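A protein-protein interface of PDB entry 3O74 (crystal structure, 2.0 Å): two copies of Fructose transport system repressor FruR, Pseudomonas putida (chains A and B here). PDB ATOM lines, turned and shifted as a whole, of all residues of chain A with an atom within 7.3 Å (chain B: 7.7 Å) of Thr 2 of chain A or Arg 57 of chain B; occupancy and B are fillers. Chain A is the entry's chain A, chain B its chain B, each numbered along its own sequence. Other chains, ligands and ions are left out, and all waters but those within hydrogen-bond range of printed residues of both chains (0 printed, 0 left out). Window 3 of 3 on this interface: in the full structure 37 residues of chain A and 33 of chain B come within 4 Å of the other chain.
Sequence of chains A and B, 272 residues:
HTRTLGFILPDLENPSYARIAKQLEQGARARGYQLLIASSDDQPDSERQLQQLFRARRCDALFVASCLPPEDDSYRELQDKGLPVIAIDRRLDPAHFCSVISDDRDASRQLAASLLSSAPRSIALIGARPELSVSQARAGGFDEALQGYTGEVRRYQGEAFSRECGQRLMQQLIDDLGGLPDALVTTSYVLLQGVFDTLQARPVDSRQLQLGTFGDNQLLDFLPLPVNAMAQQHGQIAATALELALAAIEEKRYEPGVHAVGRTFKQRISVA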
ATOM      1  N   HIS A   1      -2.090   0.738 -25.820  1.00  0.00           N
ATOM      2  CA  HIS A   1      -1.631   0.845 -24.440  1.00  0.00           C
ATOM      3  C   HIS A   1      -2.791   0.807 -23.450  1.00  0.00           C
ATOM      4  O   HIS A   1      -3.586   1.743 -23.373  1.00  0.00           O
ATOM      5  CB  HIS A   1      -0.814   2.124 -24.247  1.00  0.00           C
ATOM      6  CG  HIS A   1       0.664   1.921 -24.375  1.00  0.00           C
ATOM      7  ND1 HIS A   1       1.582   2.846 -23.928  1.00  0.00           N
ATOM      8  CD2 HIS A   1       1.379   0.894 -24.888  1.00  0.00           C
ATOM      9  CE1 HIS A   1       2.802   2.399 -24.167  1.00  0.00           C
ATOM     10  NE2 HIS A   1       2.709   1.218 -24.748  1.00  0.00           N
ATOM     11  N   THR A   2      -2.878  -0.281 -22.691  1.00  0.00           N
ATOM     12  CA  THR A   2      -3.965  -0.468 -21.735  1.00  0.00           C
ATOM     13  C   THR A   2      -3.743   0.295 -20.433  1.00  0.00           C
ATOM     14  O   THR A   2      -4.680   0.505 -19.665  1.00  0.00           O
ATOM     15  CB  THR A   2      -4.180  -1.954 -21.402  1.00  0.00           C
ATOM     16  OG1 THR A   2      -2.995  -2.492 -20.803  1.00  0.00           O
ATOM     17  CG2 THR A   2      -4.510  -2.737 -22.664  1.00  0.00           C
ATOM     18  N   ARG A   3      -2.518   0.688 -20.189  1.00  0.00           N
ATOM     19  CA  ARG A   3      -2.159   1.328 -18.954  1.00  0.00           C
ATOM     20  C   ARG A   3      -2.469   0.441 -17.764  1.00  0.00           C
ATOM     21  O   ARG A   3      -2.898   0.884 -16.760  1.00  0.00           O
ATOM     22  CB  ARG A   3      -2.860   2.641 -18.818  1.00  0.00           C
ATOM     23  CG  ARG A   3      -1.950   3.783 -18.939  1.00  0.00           C
ATOM     24  CD  ARG A   3      -1.759   4.108 -20.344  1.00  0.00           C
ATOM     25  NE  ARG A   3      -0.381   3.997 -20.757  1.00  0.00           N
ATOM     26  CZ  ARG A   3       0.381   5.024 -21.108  1.00  0.00           C
ATOM     27  NH1 ARG A   3      -0.103   6.231 -21.057  1.00  0.00           N
ATOM     28  NH2 ARG A   3       1.628   4.850 -21.491  1.00  0.00           N
ATOM     29  N   THR A   4      -2.248  -0.829 -17.924  1.00  0.00           N
ATOM     30  CA  THR A   4      -2.447  -1.769 -16.835  1.00  0.00           C
ATOM     31  C   THR A   4      -1.312  -2.782 -16.773  1.00  0.00           C
ATOM     32  O   THR A   4      -0.835  -3.268 -17.800  1.00  0.00           O
ATOM     33  CB  THR A   4      -3.796  -2.511 -16.953  1.00  0.00           C
ATOM     34  OG1 THR A   4      -3.763  -3.393 -18.081  1.00  0.00           O
ATOM     35  CG2 THR A   4      -4.938  -1.520 -17.120  1.00  0.00           C
ATOM     36  N   LEU A   5      -0.873  -3.084 -15.557  1.00  0.00           N
ATOM     37  CA  LEU A   5       0.177  -4.062 -15.345  1.00  0.00           C
ATOM     38  C   LEU A   5      -0.417  -5.293 -14.678  1.00  0.00           C
ATOM     39  O   LEU A   5      -1.379  -5.191 -13.919  1.00  0.00           O
ATOM     40  CB  LEU A   5       1.282  -3.458 -14.480  1.00  0.00           C
ATOM     41  CG  LEU A   5       1.851  -2.141 -15.022  1.00  0.00           C
ATOM     42  CD1 LEU A   5       2.715  -1.436 -13.986  1.00  0.00           C
ATOM     43  CD2 LEU A   5       2.624  -2.369 -16.317  1.00  0.00           C
ATOM     44  N   GLY A  32       0.569   6.412 -13.643  1.00  0.00           N
ATOM     45  CA  GLY A  32      -0.603   6.345 -14.500  1.00  0.00           C
ATOM     46  C   GLY A  32      -1.040   4.937 -14.860  1.00  0.00           C
ATOM     47  O   GLY A  32      -1.833   4.742 -15.785  1.00  0.00           O
ATOM     48  N   TYR A  33      -0.528   3.952 -14.129  1.00  0.00           N
ATOM     49  CA  TYR A  33      -0.843   2.553 -14.400  1.00  0.00           C
ATOM     50  C   TYR A  33      -1.713   1.905 -13.327  1.00  0.00           C
ATOM     51  O   TYR A  33      -1.638   2.254 -12.146  1.00  0.00           O
ATOM     52  CB  TYR A  33       0.442   1.741 -14.583  1.00  0.00           C
ATOM     53  CG  TYR A  33       1.160   2.014 -15.882  1.00  0.00           C
ATOM     54  CD1 TYR A  33       2.018   3.097 -16.009  1.00  0.00           C
ATOM     55  CD2 TYR A  33       0.981   1.188 -16.985  1.00  0.00           C
ATOM     56  CE1 TYR A  33       2.681   3.351 -17.197  1.00  0.00           C
ATOM     57  CE2 TYR A  33       1.640   1.433 -18.180  1.00  0.00           C
ATOM     58  CZ  TYR A  33       2.488   2.516 -18.279  1.00  0.00           C
ATOM     59  OH  TYR A  33       3.145   2.764 -19.465  1.00  0.00           O
ATOM     60  N   GLN A  34      -2.535   0.952 -13.755  1.00  0.00           N
ATOM     61  CA  GLN A  34      -3.357   0.164 -12.850  1.00  0.00           C
ATOM     62  C   GLN A  34      -2.777  -1.238 -12.748  1.00  0.00           C
ATOM     63  O   GLN A  34      -2.317  -1.798 -13.742  1.00  0.00           O
ATOM     64  CB  GLN A  34      -4.788   0.082 -13.372  1.00  0.00           C
ATOM     65  CG  GLN A  34      -5.837   0.336 -12.317  1.00  0.00           C
ATOM     66  CD  GLN A  34      -6.115   1.809 -12.125  1.00  0.00           C
ATOM     67  OE1 GLN A  34      -6.355   2.537 -13.089  1.00  0.00           O
ATOM     68  NE2 GLN A  34      -6.093   2.258 -10.876  1.00  0.00           N
ATOM     69  N   LEU A  36      -3.399  -5.234 -11.864  1.00  0.00           N
ATOM     70  CA  LEU A  36      -4.302  -6.354 -11.635  1.00  0.00           C
ATOM     71  C   LEU A  36      -3.515  -7.542 -11.093  1.00  0.00           C
ATOM     72  O   LEU A  36      -2.479  -7.920 -11.641  1.00  0.00           O
ATOM     73  CB  LEU A  36      -5.020  -6.745 -12.923  1.00  0.00           C
ATOM     74  CG  LEU A  36      -6.004  -5.734 -13.514  1.00  0.00           C
ATOM     75  CD1 LEU A  36      -6.422  -6.173 -14.913  1.00  0.00           C
ATOM     76  CD2 LEU A  36      -7.222  -5.548 -12.614  1.00  0.00           C
ATOM     77  N   ALA A  56      -4.719 -12.206 -22.759  1.00  0.00           N
ATOM     78  CA  ALA A  56      -5.921 -11.655 -23.376  1.00  0.00           C
ATOM     79  C   ALA A  56      -6.159 -10.200 -22.981  1.00  0.00           C
ATOM     80  O   ALA A  56      -6.473  -9.364 -23.827  1.00  0.00           O
ATOM     81  CB  ALA A  56      -7.134 -12.505 -23.032  1.00  0.00           C
ATOM     82  N   ARG A  57      -6.014  -9.906 -21.691  1.00  0.00           N
ATOM     83  CA  ARG A  57      -6.180  -8.547 -21.179  1.00  0.00           C
ATOM     84  C   ARG A  57      -5.251  -7.575 -21.889  1.00  0.00           C
ATOM     85  O   ARG A  57      -5.489  -6.366 -21.898  1.00  0.00           O
ATOM     86  CB  ARG A  57      -5.899  -8.510 -19.674  1.00  0.00           C
ATOM     87  CG  ARG A  57      -6.953  -9.195 -18.828  1.00  0.00           C
ATOM     88  CD  ARG A  57      -7.905  -8.179 -18.225  1.00  0.00           C
ATOM     89  NE  ARG A  57      -9.294  -8.628 -18.092  1.00  0.00           N
ATOM     90  CZ  ARG A  57      -9.751  -9.858 -18.324  1.00  0.00           C
ATOM     91  NH1 ARG A  57      -8.940 -10.836 -18.704  1.00  0.00           N
ATOM     92  NH2 ARG A  57     -11.043 -10.113 -18.164  1.00  0.00           N
ATOM     93  N   ARG A  58      -4.192  -8.116 -22.484  1.00  0.00           N
ATOM     94  CA  ARG A  58      -3.171  -7.308 -23.138  1.00  0.00           C
ATOM     95  C   ARG A  58      -2.622  -6.242 -22.188  1.00  0.00           C
ATOM     96  O   ARG A  58      -2.589  -5.058 -22.519  1.00  0.00           O
ATOM     97  CB  ARG A  58      -3.706  -6.673 -24.431  1.00  0.00           C
ATOM     98  CG  ARG A  58      -2.710  -5.773 -25.172  1.00  0.00           C
ATOM     99  CD  ARG A  58      -1.717  -6.561 -26.018  1.00  0.00           C
ATOM    100  NE  ARG A  58      -0.943  -7.522 -25.236  1.00  0.00           N
ATOM    101  CZ  ARG A  58       0.244  -7.271 -24.695  1.00  0.00           C
ATOM    102  NH1 ARG A  58       0.811  -6.081 -24.843  1.00  0.00           N
ATOM    103  NH2 ARG A  58       0.868  -8.214 -24.002  1.00  0.00           N
ATOM    104  N   CYS A  59      -2.212  -6.661 -20.995  1.00  0.00           N
ATOM    105  CA  CYS A  59      -1.548  -5.749 -20.076  1.00  0.00           C
ATOM    106  C   CYS A  59      -0.220  -5.316 -20.690  1.00  0.00           C
ATOM    107  O   CYS A  59       0.376  -6.051 -21.477  1.00  0.00           O
ATOM    108  CB  CYS A  59      -1.319  -6.416 -18.719  1.00  0.00           C
ATOM    109  SG  CYS A  59      -0.141  -7.786 -18.746  1.00  0.00           S
ATOM    110  N   ASP A  60       0.236  -4.120 -20.340  1.00  0.00           N
ATOM    111  CA  ASP A  60       1.465  -3.579 -20.912  1.00  0.00           C
ATOM    112  C   ASP A  60       2.710  -4.351 -20.470  1.00  0.00           C
ATOM    113  O   ASP A  60       3.673  -4.484 -21.227  1.00  0.00           O
ATOM    114  CB  ASP A  60       1.606  -2.097 -20.571  1.00  0.00           C
ATOM    115  CG  ASP A  60       0.480  -1.261 -21.144  1.00  0.00           C
ATOM    116  OD1 ASP A  60      -0.149  -1.704 -22.130  1.00  0.00           O
ATOM    117  OD2 ASP A  60       0.226  -0.161 -20.610  1.00  0.00           O
ATOM    118  N   ALA A  61       2.682  -4.868 -19.247  1.00  0.00           N
ATOM    119  CA  ALA A  61       3.807  -5.624 -18.713  1.00  0.00           C
ATOM    120  C   ALA A  61       3.334  -6.578 -17.623  1.00  0.00           C
ATOM    121  O   ALA A  61       2.383  -6.281 -16.906  1.00  0.00           O
ATOM    122  CB  ALA A  61       4.872  -4.683 -18.173  1.00  0.00           C
ATOM    123  N   HIS B   1     -18.902 -12.307 -22.653  1.00  0.00           N
ATOM    124  CA  HIS B   1     -18.466 -13.072 -21.487  1.00  0.00           C
ATOM    125  C   HIS B   1     -16.956 -13.314 -21.483  1.00  0.00           C
ATOM    126  O   HIS B   1     -16.361 -13.632 -22.514  1.00  0.00           O
ATOM    127  CB  HIS B   1     -19.212 -14.404 -21.415  1.00  0.00           C
ATOM    128  CG  HIS B   1     -20.479 -14.345 -20.621  1.00  0.00           C
ATOM    129  ND1 HIS B   1     -20.620 -14.965 -19.399  1.00  0.00           N
ATOM    130  CD2 HIS B   1     -21.663 -13.734 -20.870  1.00  0.00           C
ATOM    131  CE1 HIS B   1     -21.835 -14.744 -18.931  1.00  0.00           C
ATOM    132  NE2 HIS B   1     -22.488 -13.999 -19.806  1.00  0.00           N
ATOM    133  N   THR B   2     -16.341 -13.172 -20.313  1.00  0.00           N
ATOM    134  CA  THR B   2     -14.895 -13.327 -20.187  1.00  0.00           C
ATOM    135  C   THR B   2     -14.525 -14.471 -19.249  1.00  0.00           C
ATOM    136  O   THR B   2     -13.369 -14.902 -19.199  1.00  0.00           O
ATOM    137  CB  THR B   2     -14.249 -12.037 -19.654  1.00  0.00           C
ATOM    138  OG1 THR B   2     -14.826 -11.708 -18.385  1.00  0.00           O
ATOM    139  CG2 THR B   2     -14.474 -10.884 -20.619  1.00  0.00           C
ATOM    140  N   THR B   4     -14.213 -14.203 -16.188  1.00  0.00           N
ATOM    141  CA  THR B   4     -13.354 -13.647 -15.161  1.00  0.00           C
ATOM    142  C   THR B   4     -14.219 -12.833 -14.214  1.00  0.00           C
ATOM    143  O   THR B   4     -15.210 -12.222 -14.625  1.00  0.00           O
ATOM    144  CB  THR B   4     -12.251 -12.753 -15.756  1.00  0.00           C
ATOM    145  OG1 THR B   4     -12.843 -11.598 -16.360  1.00  0.00           O
ATOM    146  CG2 THR B   4     -11.462 -13.511 -16.808  1.00  0.00           C
ATOM    147  N   LEU B  36      -9.590 -11.639 -10.838  1.00  0.00           N
ATOM    148  CA  LEU B  36      -8.649 -10.532 -10.900  1.00  0.00           C
ATOM    149  C   LEU B  36      -8.881  -9.610  -9.713  1.00  0.00           C
ATOM    150  O   LEU B  36     -10.002  -9.165  -9.459  1.00  0.00           O
ATOM    151  CB  LEU B  36      -8.782  -9.762 -12.210  1.00  0.00           C
ATOM    152  CG  LEU B  36      -8.424 -10.530 -13.483  1.00  0.00           C
ATOM    153  CD1 LEU B  36      -8.743  -9.693 -14.712  1.00  0.00           C
ATOM    154  CD2 LEU B  36      -6.960 -10.946 -13.474  1.00  0.00           C
ATOM    155  N   LEU B  50     -10.761   1.938 -10.650  1.00  0.00           N
ATOM    156  CA  LEU B  50     -10.858   0.489 -10.781  1.00  0.00           C
ATOM    157  C   LEU B  50     -12.204   0.071 -11.364  1.00  0.00           C
ATOM    158  O   LEU B  50     -12.297  -0.923 -12.085  1.00  0.00           O
ATOM    159  CB  LEU B  50     -10.614  -0.199  -9.435  1.00  0.00           C
ATOM    160  CG  LEU B  50      -9.189  -0.045  -8.896  1.00  0.00           C
ATOM    161  CD1 LEU B  50      -9.036  -0.758  -7.565  1.00  0.00           C
ATOM    162  CD2 LEU B  50      -8.195  -0.581  -9.903  1.00  0.00           C
ATOM    163  N   GLN B  51     -13.246   0.835 -11.050  1.00  0.00           N
ATOM    164  CA  GLN B  51     -14.560   0.604 -11.636  1.00  0.00           C
ATOM    165  C   GLN B  51     -14.472   0.599 -13.155  1.00  0.00           C
ATOM    166  O   GLN B  51     -14.924  -0.340 -13.810  1.00  0.00           O
ATOM    167  CB  GLN B  51     -15.544   1.690 -11.203  1.00  0.00           C
ATOM    168  CG  GLN B  51     -15.965   1.622  -9.753  1.00  0.00           C
ATOM    169  CD  GLN B  51     -17.014   2.661  -9.424  1.00  0.00           C
ATOM    170  OE1 GLN B  51     -17.755   2.527  -8.451  1.00  0.00           O
ATOM    171  NE2 GLN B  51     -17.091   3.702 -10.244  1.00  0.00           N
ATOM    172  N   GLN B  52     -13.889   1.657 -13.709  1.00  0.00           N
ATOM    173  CA  GLN B  52     -13.759   1.793 -15.154  1.00  0.00           C
ATOM    174  C   GLN B  52     -12.926   0.659 -15.722  1.00  0.00           C
ATOM    175  O   GLN B  52     -13.182   0.176 -16.824  1.00  0.00           O
ATOM    176  CB  GLN B  52     -13.122   3.136 -15.513  1.00  0.00           C
ATOM    177  CG  GLN B  52     -13.991   4.332 -15.184  1.00  0.00           C
ATOM    178  CD  GLN B  52     -15.378   4.218 -15.783  1.00  0.00           C
ATOM    179  OE1 GLN B  52     -16.343   3.896 -15.087  1.00  0.00           O
ATOM    180  NE2 GLN B  52     -15.485   4.475 -17.083  1.00  0.00           N
ATOM    181  N   LEU B  53     -11.926   0.241 -14.957  1.00  0.00           N
ATOM    182  CA  LEU B  53     -11.042  -0.837 -15.371  1.00  0.00           C
ATOM    183  C   LEU B  53     -11.806  -2.147 -15.516  1.00  0.00           C
ATOM    184  O   LEU B  53     -11.721  -2.814 -16.545  1.00  0.00           O
ATOM    185  CB  LEU B  53      -9.905  -1.006 -14.365  1.00  0.00           C
ATOM    186  CG  LEU B  53      -8.888  -2.099 -14.689  1.00  0.00           C
ATOM    187  CD1 LEU B  53      -8.227  -1.820 -16.023  1.00  0.00           C
ATOM    188  CD2 LEU B  53      -7.854  -2.198 -13.584  1.00  0.00           C
ATOM    189  N   PHE B  54     -12.555  -2.513 -14.483  1.00  0.00           N
ATOM    190  CA  PHE B  54     -13.287  -3.773 -14.496  1.00  0.00           C
ATOM    191  C   PHE B  54     -14.463  -3.774 -15.462  1.00  0.00           C
ATOM    192  O   PHE B  54     -14.923  -4.835 -15.886  1.00  0.00           O
ATOM    193  CB  PHE B  54     -13.734  -4.167 -13.088  1.00  0.00           C
ATOM    194  CG  PHE B  54     -12.636  -4.768 -12.263  1.00  0.00           C
ATOM    195  CD1 PHE B  54     -12.173  -4.131 -11.126  1.00  0.00           C
ATOM    196  CD2 PHE B  54     -12.045  -5.961 -12.646  1.00  0.00           C
ATOM    197  CE1 PHE B  54     -11.154  -4.684 -10.371  1.00  0.00           C
ATOM    198  CE2 PHE B  54     -11.022  -6.522 -11.897  1.00  0.00           C
ATOM    199  CZ  PHE B  54     -10.574  -5.882 -10.757  1.00  0.00           C
ATOM    200  N   ARG B  55     -14.946  -2.585 -15.811  1.00  0.00           N
ATOM    201  CA  ARG B  55     -15.999  -2.466 -16.810  1.00  0.00           C
ATOM    202  C   ARG B  55     -15.450  -2.708 -18.216  1.00  0.00           C
ATOM    203  O   ARG B  55     -16.007  -3.490 -18.986  1.00  0.00           O
ATOM    204  CB  ARG B  55     -16.680  -1.099 -16.715  1.00  0.00           C
ATOM    205  CG  ARG B  55     -17.632  -0.801 -17.857  1.00  0.00           C
ATOM    206  CD  ARG B  55     -18.690   0.203 -17.440  1.00  0.00           C
ATOM    207  NE  ARG B  55     -18.825   1.294 -18.400  1.00  0.00           N
ATOM    208  CZ  ARG B  55     -18.508   2.558 -18.142  1.00  0.00           C
ATOM    209  NH1 ARG B  55     -18.044   2.894 -16.946  1.00  0.00           N
ATOM    210  NH2 ARG B  55     -18.663   3.486 -19.076  1.00  0.00           N
ATOM    211  N   ALA B  56     -14.346  -2.040 -18.539  1.00  0.00           N
ATOM    212  CA  ALA B  56     -13.696  -2.221 -19.832  1.00  0.00           C
ATOM    213  C   ALA B  56     -13.167  -3.645 -19.974  1.00  0.00           C
ATOM    214  O   ALA B  56     -13.220  -4.230 -21.054  1.00  0.00           O
ATOM    215  CB  ALA B  56     -12.575  -1.215 -20.006  1.00  0.00           C
ATOM    216  N   ARG B  57     -12.658  -4.192 -18.874  1.00  0.00           N
ATOM    217  CA  ARG B  57     -12.175  -5.570 -18.830  1.00  0.00           C
ATOM    218  C   ARG B  57     -13.298  -6.552 -19.137  1.00  0.00           C
ATOM    219  O   ARG B  57     -13.051  -7.684 -19.551  1.00  0.00           O
ATOM    220  CB  ARG B  57     -11.593  -5.882 -17.451  1.00  0.00           C
ATOM    221  CG  ARG B  57     -10.085  -5.821 -17.386  1.00  0.00           C
ATOM    222  CD  ARG B  57      -9.551  -4.576 -18.061  1.00  0.00           C
ATOM    223  NE  ARG B  57      -8.128  -4.701 -18.357  1.00  0.00           N
ATOM    224  CZ  ARG B  57      -7.414  -3.783 -18.999  1.00  0.00           C
ATOM    225  NH1 ARG B  57      -7.990  -2.663 -19.414  1.00  0.00           N
ATOM    226  NH2 ARG B  57      -6.124  -3.986 -19.227  1.00  0.00           N
ATOM    227  N   ARG B  58     -14.530  -6.108 -18.916  1.00  0.00           N
ATOM    228  CA  ARG B  58     -15.709  -6.935 -19.140  1.00  0.00           C
ATOM    229  C   ARG B  58     -15.778  -8.168 -18.237  1.00  0.00           C
ATOM    230  O   ARG B  58     -16.120  -9.255 -18.699  1.00  0.00           O
ATOM    231  CB  ARG B  58     -15.821  -7.344 -20.613  1.00  0.00           C
ATOM    232  CG  ARG B  58     -16.730  -6.444 -21.439  1.00  0.00           C
ATOM    233  CD  ARG B  58     -16.546  -6.670 -22.933  1.00  0.00           C
ATOM    234  NE  ARG B  58     -15.200  -6.310 -23.370  1.00  0.00           N
ATOM    235  CZ  ARG B  58     -14.250  -7.188 -23.676  1.00  0.00           C
ATOM    236  NH1 ARG B  58     -14.498  -8.488 -23.607  1.00  0.00           N
ATOM    237  NH2 ARG B  58     -13.052  -6.766 -24.059  1.00  0.00           N
ATOM    238  N   CYS B  59     -15.455  -8.008 -16.955  1.00  0.00           N
ATOM    239  CA  CYS B  59     -15.590  -9.109 -16.013  1.00  0.00           C
ATOM    240  C   CYS B  59     -17.061  -9.508 -15.897  1.00  0.00           C
ATOM    241  O   CYS B  59     -17.946  -8.664 -16.005  1.00  0.00           O
ATOM    242  CB  CYS B  59     -15.024  -8.733 -14.642  1.00  0.00           C
ATOM    243  SG  CYS B  59     -13.238  -8.448 -14.628  1.00  0.00           S
ATOM    244  N   ASP B  60     -17.317 -10.795 -15.685  1.00  0.00           N
ATOM    245  CA  ASP B  60     -18.684 -11.305 -15.632  1.00  0.00           C
ATOM    246  C   ASP B  60     -19.427 -10.855 -14.377  1.00  0.00           C
ATOM    247  O   ASP B  60     -20.652 -10.730 -14.376  1.00  0.00           O
ATOM    248  CB  ASP B  60     -18.688 -12.830 -15.737  1.00  0.00           C
ATOM    249  CG  ASP B  60     -18.197 -13.322 -17.084  1.00  0.00           C
ATOM    250  OD1 ASP B  60     -18.008 -12.481 -17.990  1.00  0.00           O
ATOM    251  OD2 ASP B  60     -18.005 -14.547 -17.235  1.00  0.00           O
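Thr 2 of chain A touches just one residue of chain B: Arg 57 (3.6 Å). Arg 57 of chain B touches three residues of chain A. No residue of chain A comes within 4 Å of Ala 56 of chain B. Of the printed residues of chain B, Thr 4 of chain A touches Leu 53 (3.5 Å) and Arg 57 (2.7 Å). Printed residues of chain B within 4 Å of Leu 36 of chain A: Leu 53 and Phe 54. Printed residues of chain A within 4 Å of Thr 4 of chain B: Arg 57 (2.9 Å). Printed residues of chain B within 4 Å of Gln 34 of chain A: Leu 50 (3.5 Å) and Leu 53 (3.5 Å). Printed residues of chain B within 4 Å of Arg 57 of chain A: Thr 4, Leu 36 and Arg 57. Ala 56 of chain A touches none of the printed residues of chain B.
Hydrophobic or aromatic side chains of chain B that line the printed part of chain A: Leu 36, Leu 50, Leu 53 and Phe 54. Of the 15 printed residues of chain A, 5 touch a printed residue of chain B. Printed residues of chain A that touch a printed residue of chain B: Thr 2, Thr 4, Gln 34, Leu 36 and Arg 57. Among the printed residues, 10 pairs touch across the chains.
The side-chain hydroxyl of Thr 4 of chain A lies within hydrogen-bond range of the guanidinium group of Arg 57 of chain B, at 2.7 Å. NH2 of Arg 57 of chain A sits at hydrogen-bond distance from OG1 of Thr 4 of chain B (2.9 Å). The backbone carbonyl oxygen (O) of Arg 57 of chain B lies within hydrogen-bond range of the guanidinium group (NH2) of Arg 57 of chain A (3.4 Å).
Thr 2 of chain A touches Arg 57 of chain B, but with the chains exchanged Arg 57 of chain A does not touch Thr 2 of chain B (4.02 Å). Thr 4 of chain A touches Arg 57 of chain B, and with the chains exchanged Arg 57 of chain A touches Thr 4 of chain B. Arg 57 of chain A touches Leu 36 of chain B, but with the chains exchanged Leu 36 of chain A does not touch Arg 57 of chain B (4.1 Å). Arg 57 of chain B touches its own counterpart, Arg 57 of chain A. Positions printed for both chains: 1, 2, 4, 36, 56, 57, 58, 59 and 60. Of the 10 pairs that touch across the chains among the printed residues, 3 have their exchanged pair printed and touching as well.
The backbone carbonyl oxygen (O) of Arg 3 of chain A lies within hydrogen-bond range of the backbone NH (N) of Gln 34 of chain A (3.0 Å). The backbone NH (N) of Asp 60 of chain A is in hydrogen-bond range of the backbone carbonyl oxygen (O) of Thr 4 of chain A, 2.9 Å away. The side-chain hydroxyl (OG1) of Thr 2 of chain B lies within hydrogen-bond range of the side-chain hydroxyl (OG1) of Thr 4 of chain B (2.8 Å). The side-chain sulfur of Cys 59 of chain B lies within hydrogen-bond range of the side-chain hydroxyl of Thr 4 of chain B (3.6 Å). O of Thr 4 of chain B sits at hydrogen-bond distance from N of Asp 60 of chain B (2.8 Å). O of Phe 54 of chain B lies within hydrogen-bond range of N of Cys 59 of chain B (3.4 Å).
CB of Thr 2 of chain A touches NH2 of Arg 57 of chain B, 3.6 Å away. Leu 53 of chain B touches Thr 4 of chain A. Gln 34 of chain A touches Leu 50 of chain B. CG of Gln 34 of chain A touches CD2 of Leu 53 of chain B (3.5 Å). Leu 36 of chain A touches Leu 53 of chain B. Leu 36 of chain A touches Phe 54 of chain B. NE of Arg 57 of chain A touches CD1 of Leu 36 of chain B, 3.6 Å away.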
